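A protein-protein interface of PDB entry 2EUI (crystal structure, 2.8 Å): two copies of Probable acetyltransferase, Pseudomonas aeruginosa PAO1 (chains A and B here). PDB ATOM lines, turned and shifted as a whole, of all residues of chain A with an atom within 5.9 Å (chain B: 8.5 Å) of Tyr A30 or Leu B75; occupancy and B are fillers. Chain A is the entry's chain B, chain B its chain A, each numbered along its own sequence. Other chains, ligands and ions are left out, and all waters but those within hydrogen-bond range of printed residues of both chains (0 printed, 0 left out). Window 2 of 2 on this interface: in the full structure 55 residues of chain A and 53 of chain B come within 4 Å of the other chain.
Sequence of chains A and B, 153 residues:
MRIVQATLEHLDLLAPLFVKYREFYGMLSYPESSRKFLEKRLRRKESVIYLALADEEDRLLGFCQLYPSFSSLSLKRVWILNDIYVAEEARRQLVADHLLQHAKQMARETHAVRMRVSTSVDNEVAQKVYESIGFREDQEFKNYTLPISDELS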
ATOM      1  N   PHE A  18       6.067 -33.768  13.010  1.00  0.00           N
ATOM      2  CA  PHE A  18       6.971 -32.979  12.187  1.00  0.00           C
ATOM      3  C   PHE A  18       8.196 -32.650  13.027  1.00  0.00           C
ATOM      4  O   PHE A  18       9.331 -32.720  12.556  1.00  0.00           O
ATOM      5  CB  PHE A  18       6.274 -31.690  11.734  1.00  0.00           C
ATOM      6  CG  PHE A  18       7.100 -30.839  10.807  1.00  0.00           C
ATOM      7  CD1 PHE A  18       7.580 -31.360   9.606  1.00  0.00           C
ATOM      8  CD2 PHE A  18       7.390 -29.512  11.125  1.00  0.00           C
ATOM      9  CE1 PHE A  18       8.336 -30.571   8.730  1.00  0.00           C
ATOM     10  CE2 PHE A  18       8.144 -28.719  10.257  1.00  0.00           C
ATOM     11  CZ  PHE A  18       8.618 -29.252   9.054  1.00  0.00           C
ATOM     12  N   VAL A  19       7.956 -32.295  14.283  1.00  0.00           N
ATOM     13  CA  VAL A  19       9.037 -31.969  15.194  1.00  0.00           C
ATOM     14  C   VAL A  19       9.908 -33.199  15.443  1.00  0.00           C
ATOM     15  O   VAL A  19      11.130 -33.084  15.496  1.00  0.00           O
ATOM     16  CB  VAL A  19       8.496 -31.443  16.550  1.00  0.00           C
ATOM     17  CG1 VAL A  19       9.646 -31.228  17.530  1.00  0.00           C
ATOM     18  CG2 VAL A  19       7.734 -30.144  16.330  1.00  0.00           C
ATOM     19  N   ARG A  22      12.355 -33.564  12.636  1.00  0.00           N
ATOM     20  CA  ARG A  22      13.490 -32.654  12.675  1.00  0.00           C
ATOM     21  C   ARG A  22      14.469 -33.088  13.768  1.00  0.00           C
ATOM     22  O   ARG A  22      15.691 -33.099  13.559  1.00  0.00           O
ATOM     23  CB  ARG A  22      13.019 -31.214  12.903  1.00  0.00           C
ATOM     24  CG  ARG A  22      12.257 -30.634  11.707  1.00  0.00           C
ATOM     25  CD  ARG A  22      11.763 -29.198  11.924  1.00  0.00           C
ATOM     26  NE  ARG A  22      12.831 -28.317  12.389  1.00  0.00           N
ATOM     27  CZ  ARG A  22      13.075 -28.059  13.669  1.00  0.00           C
ATOM     28  NH1 ARG A  22      12.321 -28.600  14.615  1.00  0.00           N
ATOM     29  NH2 ARG A  22      14.093 -27.287  14.008  1.00  0.00           N
ATOM     30  N   LEU A  28      17.254 -28.756  16.483  1.00  0.00           N
ATOM     31  CA  LEU A  28      16.695 -28.276  17.731  1.00  0.00           C
ATOM     32  C   LEU A  28      15.191 -28.176  17.544  1.00  0.00           C
ATOM     33  O   LEU A  28      14.701 -27.278  16.867  1.00  0.00           O
ATOM     34  CB  LEU A  28      17.272 -26.900  18.083  1.00  0.00           C
ATOM     35  CG  LEU A  28      18.792 -26.786  18.242  1.00  0.00           C
ATOM     36  CD1 LEU A  28      19.169 -25.330  18.465  1.00  0.00           C
ATOM     37  CD2 LEU A  28      19.270 -27.637  19.398  1.00  0.00           C
ATOM     38  N   SER A  29      14.460 -29.112  18.126  1.00  0.00           N
ATOM     39  CA  SER A  29      13.011 -29.095  18.029  1.00  0.00           C
ATOM     40  C   SER A  29      12.468 -27.732  18.426  1.00  0.00           C
ATOM     41  O   SER A  29      12.575 -27.331  19.575  1.00  0.00           O
ATOM     42  CB  SER A  29      12.426 -30.138  18.963  1.00  0.00           C
ATOM     43  OG  SER A  29      12.845 -29.894  20.291  1.00  0.00           O
ATOM     44  N   TYR A  30      11.897 -27.016  17.474  1.00  0.00           N
ATOM     45  CA  TYR A  30      11.327 -25.706  17.752  1.00  0.00           C
ATOM     46  C   TYR A  30       9.820 -25.916  17.695  1.00  0.00           C
ATOM     47  O   TYR A  30       9.170 -25.607  16.691  1.00  0.00           O
ATOM     48  CB  TYR A  30      11.766 -24.696  16.683  1.00  0.00           C
ATOM     49  CG  TYR A  30      13.135 -24.084  16.905  1.00  0.00           C
ATOM     50  CD1 TYR A  30      13.302 -22.991  17.762  1.00  0.00           C
ATOM     51  CD2 TYR A  30      14.261 -24.585  16.253  1.00  0.00           C
ATOM     52  CE1 TYR A  30      14.553 -22.410  17.963  1.00  0.00           C
ATOM     53  CE2 TYR A  30      15.523 -24.009  16.448  1.00  0.00           C
ATOM     54  CZ  TYR A  30      15.657 -22.919  17.304  1.00  0.00           C
ATOM     55  OH  TYR A  30      16.886 -22.326  17.492  1.00  0.00           O
ATOM     56  N   PRO A  31       9.243 -26.458  18.782  1.00  0.00           N
ATOM     57  CA  PRO A  31       7.813 -26.745  18.916  1.00  0.00           C
ATOM     58  C   PRO A  31       6.862 -25.751  18.254  1.00  0.00           C
ATOM     59  O   PRO A  31       6.003 -26.161  17.469  1.00  0.00           O
ATOM     60  CB  PRO A  31       7.633 -26.824  20.425  1.00  0.00           C
ATOM     61  CG  PRO A  31       8.905 -27.480  20.837  1.00  0.00           C
ATOM     62  CD  PRO A  31       9.927 -26.687  20.069  1.00  0.00           C
ATOM     63  N   GLU A  32       7.009 -24.462  18.573  1.00  0.00           N
ATOM     64  CA  GLU A  32       6.156 -23.411  18.000  1.00  0.00           C
ATOM     65  C   GLU A  32       6.559 -23.091  16.568  1.00  0.00           C
ATOM     66  O   GLU A  32       5.752 -23.196  15.643  1.00  0.00           O
ATOM     67  CB  GLU A  32       6.261 -22.106  18.789  1.00  0.00           C
ATOM     68  CG  GLU A  32       5.765 -22.122  20.209  1.00  0.00           C
ATOM     69  CD  GLU A  32       5.807 -20.722  20.828  1.00  0.00           C
ATOM     70  OE1 GLU A  32       4.985 -19.861  20.428  1.00  0.00           O
ATOM     71  OE2 GLU A  32       6.676 -20.480  21.700  1.00  0.00           O
ATOM     72  N   SER A  33       7.809 -22.677  16.398  1.00  0.00           N
ATOM     73  CA  SER A  33       8.325 -22.331  15.083  1.00  0.00           C
ATOM     74  C   SER A  33       8.040 -23.399  14.037  1.00  0.00           C
ATOM     75  O   SER A  33       7.671 -23.085  12.910  1.00  0.00           O
ATOM     76  CB  SER A  33       9.826 -22.070  15.171  1.00  0.00           C
ATOM     77  OG  SER A  33      10.060 -20.888  15.909  1.00  0.00           O
ATOM     78  N   SER A  34       8.211 -24.659  14.411  1.00  0.00           N
ATOM     79  CA  SER A  34       7.961 -25.748  13.483  1.00  0.00           C
ATOM     80  C   SER A  34       6.473 -25.788  13.125  1.00  0.00           C
ATOM     81  O   SER A  34       6.085 -26.148  12.004  1.00  0.00           O
ATOM     82  CB  SER A  34       8.388 -27.074  14.114  1.00  0.00           C
ATOM     83  OG  SER A  34       9.774 -27.071  14.403  1.00  0.00           O
ATOM     84  N   ARG A  35       5.655 -25.406  14.096  1.00  0.00           N
ATOM     85  CA  ARG A  35       4.214 -25.392  13.954  1.00  0.00           C
ATOM     86  C   ARG A  35       3.845 -24.166  13.146  1.00  0.00           C
ATOM     87  O   ARG A  35       2.978 -24.206  12.280  1.00  0.00           O
ATOM     88  CB  ARG A  35       3.589 -25.325  15.343  1.00  0.00           C
ATOM     89  CG  ARG A  35       2.141 -25.689  15.390  1.00  0.00           C
ATOM     90  CD  ARG A  35       1.270 -24.521  15.790  1.00  0.00           C
ATOM     91  NE  ARG A  35      -0.074 -25.016  16.066  1.00  0.00           N
ATOM     92  CZ  ARG A  35      -1.167 -24.260  16.084  1.00  0.00           C
ATOM     93  NH1 ARG A  35      -1.075 -22.954  15.840  1.00  0.00           N
ATOM     94  NH2 ARG A  35      -2.353 -24.815  16.330  1.00  0.00           N
ATOM     95  N   PHE A  37       5.779 -22.673  11.057  1.00  0.00           N
ATOM     96  CA  PHE A  37       6.314 -22.959   9.726  1.00  0.00           C
ATOM     97  C   PHE A  37       5.329 -23.742   8.861  1.00  0.00           C
ATOM     98  O   PHE A  37       5.144 -23.457   7.671  1.00  0.00           O
ATOM     99  CB  PHE A  37       7.593 -23.773   9.880  1.00  0.00           C
ATOM    100  CG  PHE A  37       8.257 -24.129   8.582  1.00  0.00           C
ATOM    101  CD1 PHE A  37       9.116 -23.230   7.954  1.00  0.00           C
ATOM    102  CD2 PHE A  37       8.041 -25.371   7.993  1.00  0.00           C
ATOM    103  CE1 PHE A  37       9.748 -23.566   6.759  1.00  0.00           C
ATOM    104  CE2 PHE A  37       8.670 -25.712   6.800  1.00  0.00           C
ATOM    105  CZ  PHE A  37       9.525 -24.806   6.185  1.00  0.00           C
ATOM    106  N   SER B  69      11.887 -21.473  -2.093  1.00  0.00           N
ATOM    107  CA  SER B  69      11.758 -22.782  -1.459  1.00  0.00           C
ATOM    108  C   SER B  69      12.046 -22.706   0.039  1.00  0.00           C
ATOM    109  O   SER B  69      12.260 -21.624   0.574  1.00  0.00           O
ATOM    110  CB  SER B  69      12.689 -23.802  -2.120  1.00  0.00           C
ATOM    111  OG  SER B  69      12.311 -25.124  -1.748  1.00  0.00           O
ATOM    112  N   PHE B  70      12.045 -23.855   0.709  1.00  0.00           N
ATOM    113  CA  PHE B  70      12.280 -23.899   2.155  1.00  0.00           C
ATOM    114  C   PHE B  70      13.018 -25.152   2.602  1.00  0.00           C
ATOM    115  O   PHE B  70      13.073 -26.157   1.896  1.00  0.00           O
ATOM    116  CB  PHE B  70      10.947 -23.856   2.926  1.00  0.00           C
ATOM    117  CG  PHE B  70      10.159 -22.600   2.725  1.00  0.00           C
ATOM    118  CD1 PHE B  70      10.461 -21.447   3.440  1.00  0.00           C
ATOM    119  CD2 PHE B  70       9.136 -22.553   1.790  1.00  0.00           C
ATOM    120  CE1 PHE B  70       9.758 -20.275   3.219  1.00  0.00           C
ATOM    121  CE2 PHE B  70       8.434 -21.383   1.569  1.00  0.00           C
ATOM    122  CZ  PHE B  70       8.750 -20.244   2.289  1.00  0.00           C
ATOM    123  N   SER B  71      13.575 -25.077   3.802  1.00  0.00           N
ATOM    124  CA  SER B  71      14.263 -26.200   4.415  1.00  0.00           C
ATOM    125  C   SER B  71      13.429 -26.534   5.646  1.00  0.00           C
ATOM    126  O   SER B  71      13.288 -25.710   6.551  1.00  0.00           O
ATOM    127  CB  SER B  71      15.680 -25.801   4.826  1.00  0.00           C
ATOM    128  OG  SER B  71      16.335 -26.899   5.431  1.00  0.00           O
ATOM    129  N   SER B  72      12.849 -27.725   5.673  1.00  0.00           N
ATOM    130  CA  SER B  72      12.020 -28.110   6.815  1.00  0.00           C
ATOM    131  C   SER B  72      12.887 -28.294   8.050  1.00  0.00           C
ATOM    132  O   SER B  72      12.467 -27.991   9.166  1.00  0.00           O
ATOM    133  CB  SER B  72      11.250 -29.405   6.522  1.00  0.00           C
ATOM    134  OG  SER B  72      10.277 -29.215   5.507  1.00  0.00           O
ATOM    135  N   LEU B  73      14.102 -28.780   7.836  1.00  0.00           N
ATOM    136  CA  LEU B  73      15.038 -29.006   8.916  1.00  0.00           C
ATOM    137  C   LEU B  73      15.381 -27.744   9.701  1.00  0.00           C
ATOM    138  O   LEU B  73      15.179 -27.705  10.912  1.00  0.00           O
ATOM    139  CB  LEU B  73      16.303 -29.653   8.364  1.00  0.00           C
ATOM    140  CG  LEU B  73      16.425 -31.158   8.603  1.00  0.00           C
ATOM    141  CD1 LEU B  73      15.086 -31.830   8.406  1.00  0.00           C
ATOM    142  CD2 LEU B  73      17.478 -31.741   7.679  1.00  0.00           C
ATOM    143  N   SER B  74      15.878 -26.708   9.029  1.00  0.00           N
ATOM    144  CA  SER B  74      16.246 -25.485   9.742  1.00  0.00           C
ATOM    145  C   SER B  74      15.188 -24.394   9.716  1.00  0.00           C
ATOM    146  O   SER B  74      15.458 -23.253  10.081  1.00  0.00           O
ATOM    147  CB  SER B  74      17.588 -24.925   9.231  1.00  0.00           C
ATOM    148  OG  SER B  74      17.480 -24.378   7.934  1.00  0.00           O
ATOM    149  N   LEU B  75      13.985 -24.748   9.285  1.00  0.00           N
ATOM    150  CA  LEU B  75      12.862 -23.810   9.253  1.00  0.00           C
ATOM    151  C   LEU B  75      13.207 -22.469   8.643  1.00  0.00           C
ATOM    152  O   LEU B  75      12.736 -21.433   9.099  1.00  0.00           O
ATOM    153  CB  LEU B  75      12.332 -23.587  10.669  1.00  0.00           C
ATOM    154  CG  LEU B  75      12.042 -24.874  11.428  1.00  0.00           C
ATOM    155  CD1 LEU B  75      11.819 -24.583  12.890  1.00  0.00           C
ATOM    156  CD2 LEU B  75      10.841 -25.552  10.787  1.00  0.00           C
ATOM    157  N   LYS B  76      14.027 -22.497   7.606  1.00  0.00           N
ATOM    158  CA  LYS B  76      14.430 -21.279   6.936  1.00  0.00           C
ATOM    159  C   LYS B  76      14.221 -21.366   5.415  1.00  0.00           C
ATOM    160  O   LYS B  76      13.966 -22.447   4.853  1.00  0.00           O
ATOM    161  CB  LYS B  76      15.896 -20.988   7.259  1.00  0.00           C
ATOM    162  CG  LYS B  76      16.169 -20.515   8.675  1.00  0.00           C
ATOM    163  CD  LYS B  76      17.666 -20.473   8.934  1.00  0.00           C
ATOM    164  CE  LYS B  76      18.056 -19.340   9.886  1.00  0.00           C
ATOM    165  NZ  LYS B  76      17.807 -17.972   9.308  1.00  0.00           N
ATOM    166  N   ARG B  77      14.320 -20.208   4.762  1.00  0.00           N
ATOM    167  CA  ARG B  77      14.152 -20.084   3.318  1.00  0.00           C
ATOM    168  C   ARG B  77      15.335 -20.685   2.552  1.00  0.00           C
ATOM    169  O   ARG B  77      16.419 -20.847   3.103  1.00  0.00           O
ATOM    170  CB  ARG B  77      14.007 -18.598   2.965  1.00  0.00           C
ATOM    171  CG  ARG B  77      14.233 -18.253   1.498  1.00  0.00           C
ATOM    172  CD  ARG B  77      13.011 -18.550   0.664  1.00  0.00           C
ATOM    173  NE  ARG B  77      11.928 -17.617   0.963  1.00  0.00           N
ATOM    174  CZ  ARG B  77      10.689 -17.759   0.508  1.00  0.00           C
ATOM    175  NH1 ARG B  77      10.388 -18.798  -0.257  1.00  0.00           N
ATOM    176  NH2 ARG B  77       9.758 -16.860   0.801  1.00  0.00           N
ATOM    177  N   VAL B  78      15.095 -21.032   1.291  1.00  0.00           N
ATOM    178  CA  VAL B  78      16.110 -21.564   0.387  1.00  0.00           C
ATOM    179  C   VAL B  78      15.760 -20.993  -0.982  1.00  0.00           C
ATOM    180  O   VAL B  78      14.580 -20.812  -1.297  1.00  0.00           O
ATOM    181  CB  VAL B  78      16.077 -23.100   0.261  1.00  0.00           C
ATOM    182  CG1 VAL B  78      17.008 -23.545  -0.864  1.00  0.00           C
ATOM    183  CG2 VAL B  78      16.490 -23.738   1.556  1.00  0.00           C
ATOM    184  N   HIS B 111      17.382 -13.908   4.689  1.00  0.00           N
ATOM    185  CA  HIS B 111      17.810 -14.936   5.620  1.00  0.00           C
ATOM    186  C   HIS B 111      17.628 -16.352   5.084  1.00  0.00           C
ATOM    187  O   HIS B 111      17.030 -17.208   5.743  1.00  0.00           O
ATOM    188  CB  HIS B 111      17.036 -14.758   6.927  1.00  0.00           C
ATOM    189  CG  HIS B 111      16.995 -13.339   7.398  1.00  0.00           C
ATOM    190  ND1 HIS B 111      18.118 -12.670   7.833  1.00  0.00           N
ATOM    191  CD2 HIS B 111      15.988 -12.431   7.404  1.00  0.00           C
ATOM    192  CE1 HIS B 111      17.808 -11.407   8.080  1.00  0.00           C
ATOM    193  NE2 HIS B 111      16.523 -11.236   7.826  1.00  0.00           N
ATOM    194  N   ALA B 112      18.144 -16.600   3.885  1.00  0.00           N
ATOM    195  CA  ALA B 112      18.043 -17.920   3.288  1.00  0.00           C
ATOM    196  C   ALA B 112      19.151 -18.769   3.883  1.00  0.00           C
ATOM    197  O   ALA B 112      20.216 -18.260   4.198  1.00  0.00           O
ATOM    198  CB  ALA B 112      18.209 -17.823   1.788  1.00  0.00           C
ATOM    199  N   VAL B 113      18.901 -20.059   4.062  1.00  0.00           N
ATOM    200  CA  VAL B 113      19.921 -20.943   4.611  1.00  0.00           C
ATOM    201  C   VAL B 113      20.937 -21.165   3.514  1.00  0.00           C
ATOM    202  O   VAL B 113      22.146 -21.179   3.750  1.00  0.00           O
ATOM    203  CB  VAL B 113      19.354 -22.337   4.987  1.00  0.00           C
ATOM    204  CG1 VAL B 113      20.393 -23.136   5.765  1.00  0.00           C
ATOM    205  CG2 VAL B 113      18.085 -22.186   5.781  1.00  0.00           C
ATOM    206  N   ARG B 114      20.429 -21.334   2.299  1.00  0.00           N
ATOM    207  CA  ARG B 114      21.283 -21.587   1.150  1.00  0.00           C
ATOM    208  C   ARG B 114      20.582 -21.292  -0.168  1.00  0.00           C
ATOM    209  O   ARG B 114      19.413 -20.909  -0.210  1.00  0.00           O
ATOM    210  CB  ARG B 114      21.723 -23.057   1.157  1.00  0.00           C
ATOM    211  CG  ARG B 114      20.576 -24.038   0.913  1.00  0.00           C
ATOM    212  CD  ARG B 114      21.015 -25.476   1.080  1.00  0.00           C
ATOM    213  NE  ARG B 114      21.441 -25.727   2.450  1.00  0.00           N
ATOM    214  CZ  ARG B 114      20.681 -26.278   3.393  1.00  0.00           C
ATOM    215  NH1 ARG B 114      19.438 -26.657   3.119  1.00  0.00           N
ATOM    216  NH2 ARG B 114      21.166 -26.427   4.619  1.00  0.00           N
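The guanidinium group (NE) of Arg A22 sits close to the backbone carbonyl oxygen (O) of Ser B72 (3.3 Å). O of Leu B73 lies within hydrogen-bond range of NE of Arg A22 (2.8 Å).
The backbone carbonyl oxygen of Lys B76 is in hydrogen-bond range of the backbone NH of Ser B71 (2.9 Å). NH2 of Arg A22 sits at hydrogen-bond distance from O of Leu A28 (2.9 Å). NH1 of Arg A22 lies within hydrogen-bond range of OG of Ser A34 (3.0 Å). O of Tyr A30 is in hydrogen-bond range of OG of Ser A34.
Among the printed residues, merely in contact across the chains: Ser A34 with Leu B75, Phe A18 with Ser B72, Arg A22 with Leu B75, Phe A37 with Phe B70, Phe A37 with Leu B75, Tyr A30 with Leu B75, Phe A37 with Ser B71 and Ser A33 with Leu B75.
Tyr A30 touches one residue of chain B. Of chain A, only Arg A22, Tyr A30, Ser A33, Ser A34 and Phe A37 come within 4 Å of Leu B75. Ser A29 touches none of the printed residues of chain B. No residue of chain B comes within 4 Å of Pro A31. Of the printed residues of chain B, Phe A18 touches Ser B72. Of the printed residues of chain A, Phe B70 touches Phe A37 (3.7 Å). Printed residues of chain A within 4 Å of Ser B71: Phe A37. Of the printed residues of chain A, Leu B73 touches Arg A22 (2.8 Å). Val A19 touches none of the printed residues of chain B. The nearest printed residue of chain B that does not touch Phe A18 is Leu B75 (4.2 Å).
Of the 12 printed residues of chain A, 6 touch a printed residue of chain B. Hydrophobic or aromatic side chains of chain A within 4 Å of the printed part of chain B: Phe A18, Tyr A30 and Phe A37. Among the printed residues, 10 pairs touch across the chains. Among the printed residues, no Asp or Glu carboxylate lies within 4 Å of a Lys or Arg side-chain nitrogen of the other chain.
No position is printed for both chains.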
